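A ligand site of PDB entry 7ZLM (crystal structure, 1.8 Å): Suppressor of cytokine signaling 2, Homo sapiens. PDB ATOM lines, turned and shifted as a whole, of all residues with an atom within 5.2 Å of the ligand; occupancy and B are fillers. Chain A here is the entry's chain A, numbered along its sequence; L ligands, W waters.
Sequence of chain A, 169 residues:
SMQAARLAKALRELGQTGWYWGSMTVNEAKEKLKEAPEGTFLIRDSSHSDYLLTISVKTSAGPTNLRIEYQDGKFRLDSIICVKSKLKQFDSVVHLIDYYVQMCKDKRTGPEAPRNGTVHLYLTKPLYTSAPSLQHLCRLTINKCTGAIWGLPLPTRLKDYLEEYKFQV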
ATOM      1  N   VAL A  26      14.269 -24.647  23.485  1.00  0.00           N
ATOM      2  CA  VAL A  26      15.326 -24.295  24.431  1.00  0.00           C
ATOM      3  C   VAL A  26      14.723 -23.859  25.772  1.00  0.00           C
ATOM      4  O   VAL A  26      15.242 -24.210  26.825  1.00  0.00           O
ATOM      5  CB  VAL A  26      16.254 -23.204  23.840  1.00  0.00           C
ATOM      6  CG1 VAL A  26      15.540 -21.864  23.650  1.00  0.00           C
ATOM      7  CG2 VAL A  26      17.493 -23.028  24.725  1.00  0.00           C
ATOM      8  N   ASN A  27      13.605 -23.116  25.731  1.00  0.00           N
ATOM      9  CA  ASN A  27      13.005 -22.629  26.973  1.00  0.00           C
ATOM     10  C   ASN A  27      12.454 -23.790  27.794  1.00  0.00           C
ATOM     11  O   ASN A  27      12.543 -23.786  29.036  1.00  0.00           O
ATOM     12  CB  ASN A  27      11.875 -21.641  26.679  1.00  0.00           C
ATOM     13  CG  ASN A  27      12.234 -20.676  25.560  1.00  0.00           C
ATOM     14  OD1 ASN A  27      12.308 -21.061  24.374  1.00  0.00           O
ATOM     15  ND2 ASN A  27      12.463 -19.424  25.926  1.00  0.00           N
ATOM     16  N   LYS A  30      15.345 -25.611  29.385  1.00  0.00           N
ATOM     17  CA  LYS A  30      15.852 -24.872  30.526  1.00  0.00           C
ATOM     18  C   LYS A  30      15.022 -25.145  31.768  1.00  0.00           C
ATOM     19  O   LYS A  30      15.556 -25.442  32.851  1.00  0.00           O
ATOM     20  CB  LYS A  30      15.894 -23.371  30.209  1.00  0.00           C
ATOM     21  CG  LYS A  30      16.529 -22.527  31.302  1.00  0.00           C
ATOM     22  CD  LYS A  30      16.062 -21.094  31.225  1.00  0.00           C
ATOM     23  CE  LYS A  30      14.657 -20.950  31.807  1.00  0.00           C
ATOM     24  NZ  LYS A  30      13.881 -19.792  31.261  1.00  0.00           N
ATOM     25  N   ARG A  44      17.505 -33.019  22.108  1.00  0.00           N
ATOM     26  CA  ARG A  44      16.253 -32.600  21.508  1.00  0.00           C
ATOM     27  C   ARG A  44      16.549 -32.079  20.102  1.00  0.00           C
ATOM     28  O   ARG A  44      17.710 -31.907  19.707  1.00  0.00           O
ATOM     29  CB  ARG A  44      15.578 -31.520  22.383  1.00  0.00           C
ATOM     30  CG  ARG A  44      16.497 -30.319  22.646  1.00  0.00           C
ATOM     31  CD  ARG A  44      15.854 -29.239  23.532  1.00  0.00           C
ATOM     32  NE  ARG A  44      16.776 -28.120  23.676  1.00  0.00           N
ATOM     33  CZ  ARG A  44      16.927 -27.143  22.788  1.00  0.00           C
ATOM     34  NH1 ARG A  44      16.200 -27.116  21.667  1.00  0.00           N
ATOM     35  NH2 ARG A  44      17.850 -26.220  22.989  1.00  0.00           N
ATOM     36  N   ASP A  45      15.489 -31.785  19.350  1.00  0.00           N
ATOM     37  CA  ASP A  45      15.659 -31.142  18.060  1.00  0.00           C
ATOM     38  C   ASP A  45      16.190 -29.723  18.212  1.00  0.00           C
ATOM     39  O   ASP A  45      15.889 -29.024  19.175  1.00  0.00           O
ATOM     40  CB  ASP A  45      14.323 -31.104  17.311  1.00  0.00           C
ATOM     41  CG  ASP A  45      13.813 -32.475  16.946  1.00  0.00           C
ATOM     42  OD1 ASP A  45      14.513 -33.457  17.228  1.00  0.00           O
ATOM     43  OD2 ASP A  45      12.702 -32.555  16.361  1.00  0.00           O
ATOM     44  N   SER A  46      16.963 -29.271  17.232  1.00  0.00           N
ATOM     45  CA  SER A  46      17.446 -27.885  17.232  1.00  0.00           C
ATOM     46  C   SER A  46      16.480 -26.980  16.479  1.00  0.00           C
ATOM     47  O   SER A  46      15.980 -27.335  15.408  1.00  0.00           O
ATOM     48  CB  SER A  46      18.829 -27.784  16.574  1.00  0.00           C
ATOM     49  OG  SER A  46      19.183 -26.414  16.364  1.00  0.00           O
ATOM     50  N   SER A  47      16.280 -25.763  17.011  1.00  0.00           N
ATOM     51  CA  SER A  47      15.512 -24.757  16.280  1.00  0.00           C
ATOM     52  C   SER A  47      16.198 -24.304  14.994  1.00  0.00           C
ATOM     53  O   SER A  47      15.560 -23.651  14.158  1.00  0.00           O
ATOM     54  CB  SER A  47      15.268 -23.525  17.163  1.00  0.00           C
ATOM     55  OG  SER A  47      16.410 -22.674  17.119  1.00  0.00           O
ATOM     56  N   HIS A  48      17.491 -24.591  14.820  1.00  0.00           N
ATOM     57  CA  HIS A  48      18.262 -24.021  13.723  1.00  0.00           C
ATOM     58  C   HIS A  48      18.399 -25.041  12.594  1.00  0.00           C
ATOM     59  O   HIS A  48      18.881 -26.156  12.814  1.00  0.00           O
ATOM     60  CB  HIS A  48      19.644 -23.601  14.216  1.00  0.00           C
ATOM     61  CG  HIS A  48      20.378 -22.725  13.258  1.00  0.00           C
ATOM     62  ND1 HIS A  48      20.816 -23.171  12.022  1.00  0.00           N
ATOM     63  CD2 HIS A  48      20.761 -21.426  13.350  1.00  0.00           C
ATOM     64  CE1 HIS A  48      21.439 -22.175  11.401  1.00  0.00           C
ATOM     65  NE2 HIS A  48      21.422 -21.114  12.179  1.00  0.00           N
ATOM     66  N   THR A  54      20.222 -30.797  19.432  1.00  0.00           N
ATOM     67  CA  THR A  54      20.832 -29.942  20.438  1.00  0.00           C
ATOM     68  C   THR A  54      20.969 -30.714  21.728  1.00  0.00           C
ATOM     69  O   THR A  54      20.036 -31.434  22.135  1.00  0.00           O
ATOM     70  CB  THR A  54      20.019 -28.669  20.647  1.00  0.00           C
ATOM     71  OG1 THR A  54      20.036 -27.902  19.445  1.00  0.00           O
ATOM     72  CG2 THR A  54      20.660 -27.822  21.777  1.00  0.00           C
ATOM     73  N   PRO A  63      21.248 -24.096  32.857  1.00  0.00           N
ATOM     74  CA  PRO A  63      21.255 -24.914  31.642  1.00  0.00           C
ATOM     75  C   PRO A  63      21.929 -24.186  30.482  1.00  0.00           C
ATOM     76  O   PRO A  63      21.836 -22.969  30.349  1.00  0.00           O
ATOM     77  CB  PRO A  63      19.770 -25.175  31.370  1.00  0.00           C
ATOM     78  CG  PRO A  63      19.106 -25.005  32.727  1.00  0.00           C
ATOM     79  CD  PRO A  63      19.878 -23.880  33.368  1.00  0.00           C
ATOM     80  N   THR A  64      22.636 -24.963  29.663  1.00  0.00           N
ATOM     81  CA  THR A  64      23.251 -24.442  28.464  1.00  0.00           C
ATOM     82  C   THR A  64      22.965 -25.421  27.330  1.00  0.00           C
ATOM     83  O   THR A  64      22.430 -26.510  27.565  1.00  0.00           O
ATOM     84  CB  THR A  64      24.762 -24.218  28.610  1.00  0.00           C
ATOM     85  OG1 THR A  64      25.227 -23.361  27.563  1.00  0.00           O
ATOM     86  CG2 THR A  64      25.513 -25.539  28.543  1.00  0.00           C
ATOM     87  N   ASN A  65      23.292 -25.025  26.111  1.00  0.00           N
ATOM     88  CA  ASN A  65      22.896 -25.801  24.942  1.00  0.00           C
ATOM     89  C   ASN A  65      24.044 -25.829  23.946  1.00  0.00           C
ATOM     90  O   ASN A  65      24.765 -24.848  23.775  1.00  0.00           O
ATOM     91  CB  ASN A  65      21.646 -25.185  24.268  1.00  0.00           C
ATOM     92  CG  ASN A  65      20.484 -25.031  25.228  1.00  0.00           C
ATOM     93  OD1 ASN A  65      19.624 -25.915  25.289  1.00  0.00           O
ATOM     94  ND2 ASN A  65      20.455 -23.914  26.007  1.00  0.00           N
ATOM     95  N   LEU A  66      24.182 -26.963  23.256  1.00  0.00           N
ATOM     96  CA  LEU A  66      25.262 -27.169  22.302  1.00  0.00           C
ATOM     97  C   LEU A  66      24.685 -27.960  21.128  1.00  0.00           C
ATOM     98  O   LEU A  66      24.142 -29.042  21.315  1.00  0.00           O
ATOM     99  CB  LEU A  66      26.445 -27.915  22.937  1.00  0.00           C
ATOM    100  CG  LEU A  66      27.593 -28.288  21.992  1.00  0.00           C
ATOM    101  CD1 LEU A  66      28.134 -27.043  21.284  1.00  0.00           C
ATOM    102  CD2 LEU A  66      28.688 -29.005  22.770  1.00  0.00           C
ATOM    103  N   ARG A  67      24.803 -27.407  19.926  1.00  0.00           N
ATOM    104  CA  ARG A  67      24.173 -28.057  18.783  1.00  0.00           C
ATOM    105  C   ARG A  67      25.055 -29.164  18.222  1.00  0.00           C
ATOM    106  O   ARG A  67      26.275 -29.183  18.430  1.00  0.00           O
ATOM    107  CB  ARG A  67      23.866 -27.041  17.687  1.00  0.00           C
ATOM    108  CG  ARG A  67      22.824 -26.025  18.133  1.00  0.00           C
ATOM    109  CD  ARG A  67      22.674 -24.921  17.169  1.00  0.00           C
ATOM    110  NE  ARG A  67      21.573 -24.038  17.553  1.00  0.00           N
ATOM    111  CZ  ARG A  67      21.519 -22.744  17.262  1.00  0.00           C
ATOM    112  NH1 ARG A  67      22.460 -22.155  16.531  1.00  0.00           N
ATOM    113  NH2 ARG A  67      20.469 -22.036  17.697  1.00  0.00           N
ATOM    114  N   LEU A  77      29.946 -32.200  17.078  1.00  0.00           N
ATOM    115  CA  LEU A  77      29.555 -31.008  17.808  1.00  0.00           C
ATOM    116  C   LEU A  77      29.694 -29.786  16.904  1.00  0.00           C
ATOM    117  O   LEU A  77      30.484 -29.760  15.953  1.00  0.00           O
ATOM    118  CB  LEU A  77      30.430 -30.838  19.048  1.00  0.00           C
ATOM    119  CG  LEU A  77      30.276 -31.947  20.098  1.00  0.00           C
ATOM    120  CD1 LEU A  77      31.178 -31.678  21.318  1.00  0.00           C
ATOM    121  CD2 LEU A  77      28.826 -32.076  20.514  1.00  0.00           C
ATOM    122  N   ASP A  78      28.945 -28.743  17.248  1.00  0.00           N
ATOM    123  CA  ASP A  78      28.952 -27.479  16.517  1.00  0.00           C
ATOM    124  C   ASP A  78      30.367 -26.922  16.343  1.00  0.00           C
ATOM    125  O   ASP A  78      31.066 -26.679  17.325  1.00  0.00           O
ATOM    126  CB  ASP A  78      28.074 -26.496  17.291  1.00  0.00           C
ATOM    127  CG  ASP A  78      27.748 -25.262  16.506  1.00  0.00           C
ATOM    128  OD1 ASP A  78      28.365 -24.999  15.443  1.00  0.00           O
ATOM    129  OD2 ASP A  78      26.862 -24.533  16.993  1.00  0.00           O
ATOM    130  N   ILE A  81      31.352 -23.007  17.076  1.00  0.00           N
ATOM    131  CA  ILE A  81      31.703 -22.777  18.468  1.00  0.00           C
ATOM    132  C   ILE A  81      33.071 -23.385  18.719  1.00  0.00           C
ATOM    133  O   ILE A  81      34.059 -22.670  18.916  1.00  0.00           O
ATOM    134  CB  ILE A  81      30.629 -23.405  19.381  1.00  0.00           C
ATOM    135  CG1 ILE A  81      29.307 -22.645  19.247  1.00  0.00           C
ATOM    136  CG2 ILE A  81      31.115 -23.436  20.821  1.00  0.00           C
ATOM    137  CD1 ILE A  81      28.400 -22.712  20.450  1.00  0.00           C
ATOM    138  N   CYS A  82      33.134 -24.715  18.679  1.00  0.00           N
ATOM    139  CA  CYS A  82      34.349 -25.446  18.989  1.00  0.00           C
ATOM    140  C   CYS A  82      35.275 -25.506  17.775  1.00  0.00           C
ATOM    141  O   CYS A  82      34.817 -25.501  16.628  1.00  0.00           O
ATOM    142  CB  CYS A  82      33.986 -26.862  19.458  1.00  0.00           C
ATOM    143  SG  CYS A  82      32.349 -26.988  20.321  1.00  0.00           S
ATOM    144  N   LEU A  87      37.495 -31.739  16.647  1.00  0.00           N
ATOM    145  CA  LEU A  87      36.197 -32.339  16.942  1.00  0.00           C
ATOM    146  C   LEU A  87      36.143 -33.734  16.341  1.00  0.00           C
ATOM    147  O   LEU A  87      36.348 -33.904  15.138  1.00  0.00           O
ATOM    148  CB  LEU A  87      35.064 -31.477  16.377  1.00  0.00           C
ATOM    149  CG  LEU A  87      34.806 -30.148  17.083  1.00  0.00           C
ATOM    150  CD1 LEU A  87      33.637 -29.422  16.448  1.00  0.00           C
ATOM    151  CD2 LEU A  87      34.537 -30.404  18.561  1.00  0.00           C
ATOM    152  N   HIS A 120      34.701 -27.569  26.802  1.00  0.00           N
ATOM    153  CA  HIS A 120      34.124 -27.512  28.151  1.00  0.00           C
ATOM    154  C   HIS A 120      32.668 -27.963  28.162  1.00  0.00           C
ATOM    155  O   HIS A 120      31.755 -27.217  28.522  1.00  0.00           O
ATOM    156  CB  HIS A 120      34.256 -26.107  28.732  1.00  0.00           C
ATOM    157  CG  HIS A 120      33.517 -25.050  27.962  1.00  0.00           C
ATOM    158  ND1 HIS A 120      32.264 -24.614  28.316  1.00  0.00           N
ATOM    159  CD2 HIS A 120      33.873 -24.345  26.859  1.00  0.00           C
ATOM    160  CE1 HIS A 120      31.873 -23.684  27.464  1.00  0.00           C
ATOM    161  NE2 HIS A 120      32.830 -23.501  26.569  1.00  0.00           N
ATOM    162  N   LEU A 121      32.451 -29.210  27.769  1.00  0.00           N
ATOM    163  CA  LEU A 121      31.157 -29.864  27.848  1.00  0.00           C
ATOM    164  C   LEU A 121      31.249 -30.938  28.913  1.00  0.00           C
ATOM    165  O   LEU A 121      32.028 -31.874  28.783  1.00  0.00           O
ATOM    166  CB  LEU A 121      30.770 -30.452  26.485  1.00  0.00           C
ATOM    167  CG  LEU A 121      29.561 -31.373  26.381  1.00  0.00           C
ATOM    168  CD1 LEU A 121      28.272 -30.575  26.497  1.00  0.00           C
ATOM    169  CD2 LEU A 121      29.642 -32.130  25.041  1.00  0.00           C
HETATM  170  N1  LIG L   1      23.713 -20.628  24.388  1.00  0.00           N
HETATM  171  C1  LIG L   1      24.305 -21.584  23.448  1.00  0.00           C
HETATM  172  C2  LIG L   1      25.800 -21.377  23.511  1.00  0.00           C
HETATM  173  O1  LIG L   1      26.294 -20.281  23.246  1.00  0.00           O
HETATM  174  C3  LIG L   1      23.780 -21.401  22.026  1.00  0.00           C
HETATM  175  C4  LIG L   1      22.483 -22.174  21.793  1.00  0.00           C
HETATM  176  C5  LIG L   1      22.512 -23.432  21.188  1.00  0.00           C
HETATM  177  C6  LIG L   1      21.258 -21.640  22.180  1.00  0.00           C
HETATM  178  C7  LIG L   1      21.323 -24.130  20.952  1.00  0.00           C
HETATM  179  C8  LIG L   1      20.073 -22.342  21.968  1.00  0.00           C
HETATM  180  C9  LIG L   1      20.105 -23.597  21.346  1.00  0.00           C
HETATM  181  O2  LIG L   1      18.930 -24.288  21.167  1.00  0.00           O
HETATM  182  C10 LIG L   1      22.979 -21.054  25.415  1.00  0.00           C
HETATM  183  C11 LIG L   1      22.447 -19.926  26.293  1.00  0.00           C
HETATM  184  C12 LIG L   1      21.020 -20.218  26.704  1.00  0.00           C
HETATM  185  C13 LIG L   1      19.964 -19.742  25.929  1.00  0.00           C
HETATM  186  C14 LIG L   1      18.659 -20.017  26.306  1.00  0.00           C
HETATM  187  C15 LIG L   1      18.426 -20.773  27.441  1.00  0.00           C
HETATM  188  C16 LIG L   1      19.475 -21.243  28.222  1.00  0.00           C
HETATM  189  C17 LIG L   1      20.793 -20.974  27.846  1.00  0.00           C
HETATM  190  C18 LIG L   1      27.954 -22.393  23.952  1.00  0.00           C
HETATM  191  C19 LIG L   1      28.508 -23.749  24.395  1.00  0.00           C
HETATM  192  C20 LIG L   1      28.065 -24.416  25.531  1.00  0.00           C
HETATM  193  C21 LIG L   1      28.643 -25.637  25.846  1.00  0.00           C
HETATM  194  C22 LIG L   1      29.652 -26.196  25.053  1.00  0.00           C
HETATM  195  C23 LIG L   1      30.107 -25.521  23.921  1.00  0.00           C
HETATM  196  C24 LIG L   1      31.904 -26.965  23.246  1.00  0.00           C
HETATM  197  C25 LIG L   1      32.774 -27.235  22.017  1.00  0.00           C
HETATM  198  C26 LIG L   1      29.507 -24.310  23.612  1.00  0.00           C
HETATM  199  F1  LIG L   1      17.129 -21.032  27.810  1.00  0.00           F
HETATM  200  N2  LIG L   1      26.497 -22.443  23.874  1.00  0.00           N
HETATM  201  N3  LIG L   1      31.037 -25.952  23.045  1.00  0.00           N
HETATM  202  O3  LIG L   1      22.718 -22.232  25.644  1.00  0.00           O
HETATM  203  O4  LIG L   1      32.054 -27.619  24.277  1.00  0.00           O
HETATM  204  O5  LIG L   1      16.960 -25.149  19.893  1.00  0.00           O
HETATM  205  O6  LIG L   1      19.419 -25.389  18.906  1.00  0.00           O
HETATM  206  O7  LIG L   1      18.265 -23.112  19.003  1.00  0.00           O
HETATM  207  P1  LIG L   1      18.345 -24.471  19.657  1.00  0.00           P
HETATM  208  O   HOH W   1      28.388 -18.854  24.558  1.00  0.00           O
HETATM  209  O   HOH W   2      14.732 -24.043  20.690  1.00  0.00           O
HETATM  210  O   HOH W   3      23.316 -19.908  18.958  1.00  0.00           O
HETATM  211  O   HOH W   4      25.242 -21.978  18.959  1.00  0.00           O
HETATM  212  O   HOH W   5      24.974 -20.953  28.453  1.00  0.00           O
HETATM  213  O   HOH W   6      17.058 -20.946  20.166  1.00  0.00           O
HETATM  214  O   HOH W   7      20.992 -19.191  19.757  1.00  0.00           O
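The side-chain sulfur (SG) of Cys 82 is bonded to a carbon (C25) of the ligand, 1.8 Å away. OG1 of Thr 54 lies within hydrogen-bond range of O6 of the ligand (2.6 Å). An oxygen (O5) of the ligand lies within hydrogen-bond range of the backbone NH of Ser 47, 3.0 Å away. An oxygen (O7) of the ligand sits at hydrogen-bond distance from the side-chain hydroxyl (OG) of Ser 47 (2.7 Å). OG of Ser 46 sits at hydrogen-bond distance from O6 of the ligand. The guanidinium group of Arg 44 is in salt-bridge range of an oxygen (O5) of the ligand (2.8 Å). NH2 of Arg 67 lies within salt-bridge range of O7 of the ligand (2.8 Å). N of Asn 65 sits at hydrogen-bond distance from O3 of the ligand. O of Asn 65 sits at hydrogen-bond distance from N2 of the ligand. The side-chain amide nitrogen (ND2) of Asn 65 sits at hydrogen-bond distance from an oxygen (O3) of the ligand (2.8 Å). The side-chain hydroxyl (OG1) of Thr 64 is in hydrogen-bond range of an oxygen (O3) of the ligand, at 3.4 Å.
Val 26 touches the ligand. Lys 30 touches the ligand. Pro 63 touches the ligand. Leu 66 touches the ligand (CD1 to N3, 3.6 Å). Ile 81 touches the ligand (CG2 to C26, 3.3 Å). N of His 120 touches O4 of the ligand, at 3.7 Å. CB of Leu 121 touches O4 of the ligand, 3.8 Å away. Hydrophobic or aromatic side chains within 4 Å of the ligand: Val 26, Leu 66, Ile 81 and Leu 121. Within 4 Å of the ligand: Val 26, Lys 30, Arg 44, Ser 46, Ser 47, Thr 54, Pro 63, Thr 64, Asn 65, Leu 66, Arg 67, Ile 81, Cys 82, His 120 and Leu 121. Along chain A the residues within 4 Å of the ligand span positions 26 to 121. The nearest printed residue that does not touch the ligand is Asp 45 (4.1 Å).
Water W2 lies within hydrogen-bond range of an oxygen (O5) of the ligand (2.6 Å) and the backbone NH (N) of Val 26 (2.9 Å).
The backbone NH (N) of Thr 54 lies within hydrogen-bond range of the backbone carbonyl oxygen (O) of Arg 44, at 2.8 Å. The backbone NH (N) of His 48 lies within hydrogen-bond range of the side-chain hydroxyl (OG) of Ser 46. The side-chain amide oxygen (OD1) of Asn 65 sits at hydrogen-bond distance from the guanidinium group (NH2) of Arg 44. O of Arg 67 is in hydrogen-bond range of N of Asp 78 (3.0 Å).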
